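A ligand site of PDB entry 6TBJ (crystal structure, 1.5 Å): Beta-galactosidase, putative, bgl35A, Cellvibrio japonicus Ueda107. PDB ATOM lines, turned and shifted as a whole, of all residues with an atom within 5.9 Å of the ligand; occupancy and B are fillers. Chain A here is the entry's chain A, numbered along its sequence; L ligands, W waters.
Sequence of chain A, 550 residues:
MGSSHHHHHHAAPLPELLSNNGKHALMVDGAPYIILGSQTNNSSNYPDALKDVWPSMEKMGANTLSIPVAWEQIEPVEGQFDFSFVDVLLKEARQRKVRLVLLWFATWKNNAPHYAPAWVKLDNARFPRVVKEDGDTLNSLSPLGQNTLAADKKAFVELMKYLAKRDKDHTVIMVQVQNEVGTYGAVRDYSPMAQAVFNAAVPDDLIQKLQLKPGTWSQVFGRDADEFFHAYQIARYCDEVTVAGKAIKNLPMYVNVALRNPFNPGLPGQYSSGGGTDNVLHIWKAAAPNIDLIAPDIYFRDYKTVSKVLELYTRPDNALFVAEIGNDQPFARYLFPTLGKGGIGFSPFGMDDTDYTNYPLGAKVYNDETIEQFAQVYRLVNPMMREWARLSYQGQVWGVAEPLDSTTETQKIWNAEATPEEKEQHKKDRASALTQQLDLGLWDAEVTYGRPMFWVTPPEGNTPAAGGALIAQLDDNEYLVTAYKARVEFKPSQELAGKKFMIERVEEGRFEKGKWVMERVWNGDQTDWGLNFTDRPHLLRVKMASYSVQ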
ATOM      1  N   GLN A  39     -28.984  20.530 -36.596  1.00  0.00           N
ATOM      2  CA  GLN A  39     -28.301  21.783 -36.978  1.00  0.00           C
ATOM      3  C   GLN A  39     -27.199  21.407 -37.947  1.00  0.00           C
ATOM      4  O   GLN A  39     -26.440  20.465 -37.730  1.00  0.00           O
ATOM      5  CB  GLN A  39     -27.723  22.555 -35.791  1.00  0.00           C
ATOM      6  CG  GLN A  39     -26.913  23.766 -36.216  1.00  0.00           C
ATOM      7  CD  GLN A  39     -26.551  24.837 -35.206  1.00  0.00           C
ATOM      8  OE1 GLN A  39     -25.710  25.679 -35.487  1.00  0.00           O
ATOM      9  NE2 GLN A  39     -27.167  24.877 -34.031  1.00  0.00           N
ATOM     10  N   ASN A  42     -21.236  24.756 -39.612  1.00  0.00           N
ATOM     11  CA  ASN A  42     -21.153  26.217 -39.736  1.00  0.00           C
ATOM     12  C   ASN A  42     -20.989  26.758 -41.166  1.00  0.00           C
ATOM     13  O   ASN A  42     -21.114  27.980 -41.340  1.00  0.00           O
ATOM     14  CB  ASN A  42     -19.952  26.717 -38.918  1.00  0.00           C
ATOM     15  CG  ASN A  42     -20.132  26.668 -37.404  1.00  0.00           C
ATOM     16  OD1 ASN A  42     -19.140  26.856 -36.706  1.00  0.00           O
ATOM     17  ND2 ASN A  42     -21.313  26.409 -36.872  1.00  0.00           N
ATOM     18  N   PHE A 105     -25.847  34.983 -37.429  1.00  0.00           N
ATOM     19  CA  PHE A 105     -24.397  35.018 -37.147  1.00  0.00           C
ATOM     20  C   PHE A 105     -23.912  36.421 -37.516  1.00  0.00           C
ATOM     21  O   PHE A 105     -23.891  36.719 -38.699  1.00  0.00           O
ATOM     22  CB  PHE A 105     -23.652  33.982 -37.961  1.00  0.00           C
ATOM     23  CG  PHE A 105     -23.736  32.549 -37.519  1.00  0.00           C
ATOM     24  CD1 PHE A 105     -24.648  32.100 -36.562  1.00  0.00           C
ATOM     25  CD2 PHE A 105     -22.836  31.620 -38.036  1.00  0.00           C
ATOM     26  CE1 PHE A 105     -24.682  30.762 -36.170  1.00  0.00           C
ATOM     27  CE2 PHE A 105     -22.890  30.276 -37.695  1.00  0.00           C
ATOM     28  CZ  PHE A 105     -23.823  29.848 -36.742  1.00  0.00           C
ATOM     29  N   LYS A 109     -20.157  35.343 -33.093  1.00  0.00           N
ATOM     30  CA  LYS A 109     -20.244  33.913 -33.408  1.00  0.00           C
ATOM     31  C   LYS A 109     -19.072  33.262 -32.692  1.00  0.00           C
ATOM     32  O   LYS A 109     -17.958  33.531 -33.080  1.00  0.00           O
ATOM     33  CB  LYS A 109     -20.278  33.685 -34.925  1.00  0.00           C
ATOM     34  CG  LYS A 109     -20.701  32.294 -35.359  1.00  0.00           C
ATOM     35  CD  LYS A 109     -19.694  31.221 -35.031  1.00  0.00           C
ATOM     36  CE  LYS A 109     -20.026  29.817 -35.486  1.00  0.00           C
ATOM     37  NZ  LYS A 109     -19.199  28.807 -34.785  1.00  0.00           N
ATOM     38  N   ASN A 110     -19.364  32.540 -31.612  1.00  0.00           N
ATOM     39  CA  ASN A 110     -18.339  31.977 -30.695  1.00  0.00           C
ATOM     40  C   ASN A 110     -17.367  33.087 -30.242  1.00  0.00           C
ATOM     41  O   ASN A 110     -16.174  32.909 -30.479  1.00  0.00           O
ATOM     42  CB  ASN A 110     -17.548  30.793 -31.288  1.00  0.00           C
ATOM     43  CG  ASN A 110     -18.431  29.576 -31.594  1.00  0.00           C
ATOM     44  OD1 ASN A 110     -19.632  29.690 -31.871  1.00  0.00           O
ATOM     45  ND2 ASN A 110     -17.826  28.399 -31.595  1.00  0.00           N
ATOM     46  N   ASN A 179     -24.604  34.069 -31.961  1.00  0.00           N
ATOM     47  CA  ASN A 179     -24.284  32.634 -31.764  1.00  0.00           C
ATOM     48  C   ASN A 179     -23.218  32.588 -30.683  1.00  0.00           C
ATOM     49  O   ASN A 179     -22.124  33.042 -30.980  1.00  0.00           O
ATOM     50  CB  ASN A 179     -23.821  31.945 -33.065  1.00  0.00           C
ATOM     51  CG  ASN A 179     -23.578  30.474 -32.818  1.00  0.00           C
ATOM     52  OD1 ASN A 179     -24.508  29.705 -32.695  1.00  0.00           O
ATOM     53  ND2 ASN A 179     -22.308  30.096 -32.770  1.00  0.00           N
ATOM     54  N   GLU A 180     -23.528  32.187 -29.464  1.00  0.00           N
ATOM     55  CA  GLU A 180     -22.503  32.071 -28.385  1.00  0.00           C
ATOM     56  C   GLU A 180     -21.750  33.418 -28.189  1.00  0.00           C
ATOM     57  O   GLU A 180     -20.578  33.550 -28.557  1.00  0.00           O
ATOM     58  CB  GLU A 180     -21.620  30.859 -28.670  1.00  0.00           C
ATOM     59  CG  GLU A 180     -22.346  29.558 -28.449  1.00  0.00           C
ATOM     60  CD  GLU A 180     -21.515  28.265 -28.421  1.00  0.00           C
ATOM     61  OE1 GLU A 180     -20.303  28.312 -28.534  1.00  0.00           O
ATOM     62  OE2 GLU A 180     -22.091  27.229 -28.165  1.00  0.00           O
ATOM     63  N   TYR A 184     -13.600  35.352 -24.986  1.00  0.00           N
ATOM     64  CA  TYR A 184     -12.561  34.473 -24.436  1.00  0.00           C
ATOM     65  C   TYR A 184     -11.314  35.337 -24.286  1.00  0.00           C
ATOM     66  O   TYR A 184     -11.019  36.112 -25.251  1.00  0.00           O
ATOM     67  CB  TYR A 184     -12.249  33.331 -25.387  1.00  0.00           C
ATOM     68  CG  TYR A 184     -13.331  32.299 -25.542  1.00  0.00           C
ATOM     69  CD1 TYR A 184     -13.744  31.533 -24.473  1.00  0.00           C
ATOM     70  CD2 TYR A 184     -13.957  32.123 -26.761  1.00  0.00           C
ATOM     71  CE1 TYR A 184     -14.729  30.580 -24.602  1.00  0.00           C
ATOM     72  CE2 TYR A 184     -14.932  31.152 -26.916  1.00  0.00           C
ATOM     73  CZ  TYR A 184     -15.325  30.367 -25.829  1.00  0.00           C
ATOM     74  OH  TYR A 184     -16.291  29.396 -25.926  1.00  0.00           O
ATOM     75  N   ASN A 256     -28.161  31.453 -27.487  1.00  0.00           N
ATOM     76  CA  ASN A 256     -27.543  30.131 -27.177  1.00  0.00           C
ATOM     77  C   ASN A 256     -26.235  30.352 -26.426  1.00  0.00           C
ATOM     78  O   ASN A 256     -25.341  31.082 -26.933  1.00  0.00           O
ATOM     79  CB  ASN A 256     -27.318  29.281 -28.432  1.00  0.00           C
ATOM     80  CG  ASN A 256     -26.407  29.914 -29.454  1.00  0.00           C
ATOM     81  OD1 ASN A 256     -26.383  31.113 -29.579  1.00  0.00           O
ATOM     82  ND2 ASN A 256     -25.586  29.076 -30.129  1.00  0.00           N
ATOM     83  N   LEU A 259     -21.495  27.124 -22.677  1.00  0.00           N
ATOM     84  CA  LEU A 259     -21.691  26.796 -21.267  1.00  0.00           C
ATOM     85  C   LEU A 259     -20.333  26.887 -20.591  1.00  0.00           C
ATOM     86  O   LEU A 259     -19.362  26.389 -21.132  1.00  0.00           O
ATOM     87  CB  LEU A 259     -22.279  25.392 -21.089  1.00  0.00           C
ATOM     88  CG  LEU A 259     -23.666  25.221 -21.701  1.00  0.00           C
ATOM     89  CD1 LEU A 259     -24.075  23.765 -21.649  1.00  0.00           C
ATOM     90  CD2 LEU A 259     -24.678  26.157 -21.071  1.00  0.00           C
ATOM     91  N   ASN A 261     -18.652  24.935 -17.247  1.00  0.00           N
ATOM     92  CA  ASN A 261     -18.925  23.721 -16.473  1.00  0.00           C
ATOM     93  C   ASN A 261     -19.676  24.123 -15.199  1.00  0.00           C
ATOM     94  O   ASN A 261     -19.242  24.993 -14.453  1.00  0.00           O
ATOM     95  CB  ASN A 261     -17.629  22.983 -16.209  1.00  0.00           C
ATOM     96  CG  ASN A 261     -17.904  21.648 -15.569  1.00  0.00           C
ATOM     97  OD1 ASN A 261     -18.380  21.607 -14.432  1.00  0.00           O
ATOM     98  ND2 ASN A 261     -17.656  20.578 -16.297  1.00  0.00           N
ATOM     99  N   ASP A 297     -25.909  25.019 -24.912  1.00  0.00           N
ATOM    100  CA  ASP A 297     -25.227  24.266 -25.999  1.00  0.00           C
ATOM    101  C   ASP A 297     -24.402  23.177 -25.332  1.00  0.00           C
ATOM    102  O   ASP A 297     -23.376  23.530 -24.729  1.00  0.00           O
ATOM    103  CB  ASP A 297     -24.363  25.214 -26.847  1.00  0.00           C
ATOM    104  CG  ASP A 297     -25.156  26.248 -27.606  1.00  0.00           C
ATOM    105  OD1 ASP A 297     -26.401  26.133 -27.680  1.00  0.00           O
ATOM    106  OD2 ASP A 297     -24.530  27.218 -28.086  1.00  0.00           O
ATOM    107  N   ILE A 298     -24.828  21.908 -25.395  1.00  0.00           N
ATOM    108  CA  ILE A 298     -24.362  20.855 -24.470  1.00  0.00           C
ATOM    109  C   ILE A 298     -23.364  19.953 -25.169  1.00  0.00           C
ATOM    110  O   ILE A 298     -23.732  19.258 -26.110  1.00  0.00           O
ATOM    111  CB  ILE A 298     -25.572  20.104 -23.896  1.00  0.00           C
ATOM    112  CG1 ILE A 298     -26.550  21.062 -23.209  1.00  0.00           C
ATOM    113  CG2 ILE A 298     -25.047  18.965 -23.014  1.00  0.00           C
ATOM    114  CD1 ILE A 298     -27.749  20.315 -22.656  1.00  0.00           C
ATOM    115  N   TYR A 299     -22.135  19.923 -24.673  1.00  0.00           N
ATOM    116  CA  TYR A 299     -21.083  19.041 -25.228  1.00  0.00           C
ATOM    117  C   TYR A 299     -20.394  18.267 -24.100  1.00  0.00           C
ATOM    118  O   TYR A 299     -19.530  17.429 -24.409  1.00  0.00           O
ATOM    119  CB  TYR A 299     -20.082  19.789 -26.093  1.00  0.00           C
ATOM    120  CG  TYR A 299     -20.745  20.398 -27.300  1.00  0.00           C
ATOM    121  CD1 TYR A 299     -21.414  21.622 -27.238  1.00  0.00           C
ATOM    122  CD2 TYR A 299     -20.828  19.647 -28.472  1.00  0.00           C
ATOM    123  CE1 TYR A 299     -22.070  22.137 -28.347  1.00  0.00           C
ATOM    124  CE2 TYR A 299     -21.405  20.189 -29.608  1.00  0.00           C
ATOM    125  CZ  TYR A 299     -22.042  21.430 -29.553  1.00  0.00           C
ATOM    126  OH  TYR A 299     -22.677  21.901 -30.678  1.00  0.00           O
ATOM    127  N   PHE A 300     -20.838  18.443 -22.851  1.00  0.00           N
ATOM    128  CA  PHE A 300     -20.355  17.635 -21.704  1.00  0.00           C
ATOM    129  C   PHE A 300     -20.782  16.194 -21.968  1.00  0.00           C
ATOM    130  O   PHE A 300     -21.947  16.004 -22.343  1.00  0.00           O
ATOM    131  CB  PHE A 300     -20.927  18.145 -20.382  1.00  0.00           C
ATOM    132  CG  PHE A 300     -20.672  19.594 -20.087  1.00  0.00           C
ATOM    133  CD1 PHE A 300     -19.389  20.103 -19.985  1.00  0.00           C
ATOM    134  CD2 PHE A 300     -21.722  20.495 -19.940  1.00  0.00           C
ATOM    135  CE1 PHE A 300     -19.172  21.444 -19.730  1.00  0.00           C
ATOM    136  CE2 PHE A 300     -21.499  21.841 -19.714  1.00  0.00           C
ATOM    137  CZ  PHE A 300     -20.222  22.329 -19.639  1.00  0.00           C
ATOM    138  N   ARG A 301     -19.916  15.213 -21.739  1.00  0.00           N
ATOM    139  CA  ARG A 301     -20.314  13.819 -22.064  1.00  0.00           C
ATOM    140  C   ARG A 301     -20.946  13.125 -20.860  1.00  0.00           C
ATOM    141  O   ARG A 301     -21.841  12.243 -21.078  1.00  0.00           O
ATOM    142  CB  ARG A 301     -19.121  13.019 -22.563  1.00  0.00           C
ATOM    143  CG  ARG A 301     -18.913  13.234 -24.052  1.00  0.00           C
ATOM    144  CD  ARG A 301     -17.515  13.257 -24.571  1.00  0.00           C
ATOM    145  NE  ARG A 301     -17.498  13.478 -26.016  1.00  0.00           N
ATOM    146  CZ  ARG A 301     -17.913  12.617 -26.940  1.00  0.00           C
ATOM    147  NH1 ARG A 301     -18.388  11.428 -26.609  1.00  0.00           N
ATOM    148  NH2 ARG A 301     -17.793  12.948 -28.227  1.00  0.00           N
ATOM    149  N   GLU A 324     -28.240  23.262 -28.987  1.00  0.00           N
ATOM    150  CA  GLU A 324     -27.157  22.474 -29.565  1.00  0.00           C
ATOM    151  C   GLU A 324     -26.808  21.323 -28.629  1.00  0.00           C
ATOM    152  O   GLU A 324     -26.851  21.503 -27.440  1.00  0.00           O
ATOM    153  CB  GLU A 324     -25.880  23.275 -29.713  1.00  0.00           C
ATOM    154  CG  GLU A 324     -25.880  24.315 -30.778  1.00  0.00           C
ATOM    155  CD  GLU A 324     -24.544  25.022 -30.803  1.00  0.00           C
ATOM    156  OE1 GLU A 324     -23.500  24.390 -30.447  1.00  0.00           O
ATOM    157  OE2 GLU A 324     -24.542  26.211 -31.043  1.00  0.00           O
ATOM    158  N   PHE A 349     -25.940  18.913 -33.183  1.00  0.00           N
ATOM    159  CA  PHE A 349     -25.127  19.819 -34.029  1.00  0.00           C
ATOM    160  C   PHE A 349     -24.282  19.051 -35.040  1.00  0.00           C
ATOM    161  O   PHE A 349     -23.692  18.095 -34.632  1.00  0.00           O
ATOM    162  CB  PHE A 349     -24.175  20.609 -33.148  1.00  0.00           C
ATOM    163  CG  PHE A 349     -23.314  21.554 -33.917  1.00  0.00           C
ATOM    164  CD1 PHE A 349     -23.736  22.837 -34.246  1.00  0.00           C
ATOM    165  CD2 PHE A 349     -22.108  21.114 -34.429  1.00  0.00           C
ATOM    166  CE1 PHE A 349     -22.971  23.646 -35.069  1.00  0.00           C
ATOM    167  CE2 PHE A 349     -21.318  21.935 -35.217  1.00  0.00           C
ATOM    168  CZ  PHE A 349     -21.744  23.225 -35.490  1.00  0.00           C
ATOM    169  N   TYR A 356     -17.040  17.279 -42.588  1.00  0.00           N
ATOM    170  CA  TYR A 356     -16.525  17.907 -41.366  1.00  0.00           C
ATOM    171  C   TYR A 356     -17.113  17.194 -40.150  1.00  0.00           C
ATOM    172  O   TYR A 356     -18.271  16.745 -40.150  1.00  0.00           O
ATOM    173  CB  TYR A 356     -16.859  19.375 -41.261  1.00  0.00           C
ATOM    174  CG  TYR A 356     -16.189  20.028 -40.061  1.00  0.00           C
ATOM    175  CD1 TYR A 356     -14.895  20.526 -40.150  1.00  0.00           C
ATOM    176  CD2 TYR A 356     -16.832  20.174 -38.835  1.00  0.00           C
ATOM    177  CE1 TYR A 356     -14.230  21.104 -39.069  1.00  0.00           C
ATOM    178  CE2 TYR A 356     -16.193  20.797 -37.762  1.00  0.00           C
ATOM    179  CZ  TYR A 356     -14.875  21.229 -37.849  1.00  0.00           C
ATOM    180  OH  TYR A 356     -14.220  21.790 -36.752  1.00  0.00           O
ATOM    181  N   ASN A 358     -16.820  17.687 -35.694  1.00  0.00           N
ATOM    182  CA  ASN A 358     -16.257  18.504 -34.598  1.00  0.00           C
ATOM    183  C   ASN A 358     -15.726  17.570 -33.498  1.00  0.00           C
ATOM    184  O   ASN A 358     -15.462  18.085 -32.386  1.00  0.00           O
ATOM    185  CB  ASN A 358     -17.207  19.562 -34.021  1.00  0.00           C
ATOM    186  CG  ASN A 358     -18.442  19.043 -33.327  1.00  0.00           C
ATOM    187  OD1 ASN A 358     -18.695  17.860 -33.253  1.00  0.00           O
ATOM    188  ND2 ASN A 358     -19.302  19.943 -32.925  1.00  0.00           N
ATOM    189  N   LEU A 361     -15.625  16.908 -29.831  1.00  0.00           N
ATOM    190  CA  LEU A 361     -16.981  17.276 -29.327  1.00  0.00           C
ATOM    191  C   LEU A 361     -18.054  16.310 -29.818  1.00  0.00           C
ATOM    192  O   LEU A 361     -18.901  15.904 -29.040  1.00  0.00           O
ATOM    193  CB  LEU A 361     -17.342  18.697 -29.768  1.00  0.00           C
ATOM    194  CG  LEU A 361     -16.447  19.786 -29.211  1.00  0.00           C
ATOM    195  CD1 LEU A 361     -17.007  21.155 -29.566  1.00  0.00           C
ATOM    196  CD2 LEU A 361     -16.222  19.644 -27.710  1.00  0.00           C
HETATM  197  C1  LIG L   1     -15.967  19.053 -23.164  1.00  0.00           C
HETATM  198  N1  LIG L   1     -16.067  21.689 -23.675  1.00  0.00           N
HETATM  199  C2  LIG L   1     -16.536  23.546 -25.316  1.00  0.00           C
HETATM  200  C3  LIG L   1     -16.700  23.871 -26.813  1.00  0.00           C
HETATM  201  C4  LIG L   1     -18.169  23.705 -27.310  1.00  0.00           C
HETATM  202  C5  LIG L   1     -18.310  24.586 -28.543  1.00  0.00           C
HETATM  203  C6  LIG L   1     -19.581  24.267 -29.322  1.00  0.00           C
HETATM  204  C7  LIG L   1     -19.834  25.156 -30.571  1.00  0.00           C
HETATM  205  N2  LIG L   1     -21.140  25.805 -30.376  1.00  0.00           N
HETATM  206  C8  LIG L   1     -21.341  26.820 -31.436  1.00  0.00           C
HETATM  207  C9  LIG L   1     -21.425  26.076 -32.773  1.00  0.00           C
HETATM  208  O1  LIG L   1     -21.642  27.018 -33.855  1.00  0.00           O
HETATM  209  C10 LIG L   1     -20.144  25.288 -33.040  1.00  0.00           C
HETATM  210  O2  LIG L   1     -19.056  26.233 -33.209  1.00  0.00           O
HETATM  211  C11 LIG L   1     -19.884  24.378 -31.867  1.00  0.00           C
HETATM  212  C12 LIG L   1     -18.581  23.577 -32.037  1.00  0.00           C
HETATM  213  O3  LIG L   1     -18.726  22.736 -33.175  1.00  0.00           O
HETATM  214  C13 LIG L   1     -16.717  22.052 -24.958  1.00  0.00           C
HETATM  215  S1  LIG L   1     -16.721  20.435 -22.891  1.00  0.00           S
HETATM  216  O4  LIG L   1     -18.093  20.305 -23.207  1.00  0.00           O
HETATM  217  O5  LIG L   1     -16.651  20.681 -21.474  1.00  0.00           O
HETATM  218  O   HOH W   1     -20.791  21.920 -23.230  1.00  0.00           O
HETATM  219  O   HOH W   2     -24.125  27.400 -34.367  1.00  0.00           O
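N2 of the ligand lies within salt-bridge range of OE1 of Glu 324, 2.8 Å away. OE2 of Glu 180 lies within salt-bridge range of N2 of the ligand (2.8 Å). The side-chain amide nitrogen (ND2) of Asn 358 is in hydrogen-bond range of an oxygen (O3) of the ligand, 2.9 Å away. ND2 of Asn 110 sits at hydrogen-bond distance from O2 of the ligand, at 3.0 Å. O2 of the ligand lies within hydrogen-bond range of NZ of Lys 109. The side-chain amide nitrogen of Asn 42 is in hydrogen-bond range of an oxygen (O1) of the ligand, 3.1 Å away. The backbone NH (N) of Phe 300 is in hydrogen-bond range of an oxygen (O4) of the ligand (3.3 Å). The side-chain amide nitrogen (ND2) of Asn 179 lies within hydrogen-bond range of an oxygen (O1) of the ligand (3.3 Å).
The side-chain carboxylate (OE2) of Glu 324 sits at hydrogen-bond distance from the side-chain amide nitrogen (ND2) of Asn 256 (3.2 Å). N of Ile 298 sits at hydrogen-bond distance from O of Glu 324 (2.9 Å). The backbone carbonyl oxygen of Glu 180 lies within hydrogen-bond range of the backbone NH of Asn 110. The side-chain carboxylate (OE2) of Glu 180 sits close to the side-chain carboxylate (OD2) of Asp 297 (2.4 Å). OD1 of Asn 110 sits at hydrogen-bond distance from NZ of Lys 109 (3.1 Å). ND2 of Asn 179 lies within hydrogen-bond range of OD1 of Asn 110 (2.9 Å). The side-chain amide oxygen (OD1) of Asn 42 is in hydrogen-bond range of the side-chain amino group (NZ) of Lys 109, 2.7 Å away. The backbone carbonyl oxygen (O) of Leu 361 is in hydrogen-bond range of the guanidinium group (NH2) of Arg 301, 3.3 Å away.
O4 of the ligand lies close to O of Tyr 299, at 3.4 Å. Phe 349 touches the ligand (CE2 to O3, 3.4 Å). Leu 361 touches the ligand. Along chain A the residues within 4 Å of the ligand span positions 42 to 361. The nearest printed residue that does not touch the ligand is Asp 297 (4.3 Å).
Water W2 lies within hydrogen-bond range of O1 of the ligand (2.6 Å), OE1 of Gln 39 (2.6 Å) and OD1 of Asn 179 (2.9 Å). Water W1 lies within hydrogen-bond range of the backbone NH (N) of Tyr 299 (2.8 Å), an oxygen (O4) of the ligand (3.1 Å), the backbone carbonyl oxygen (O) of Asp 297 (3.4 Å) and the backbone NH (N) of Phe 300 (3.5 Å).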
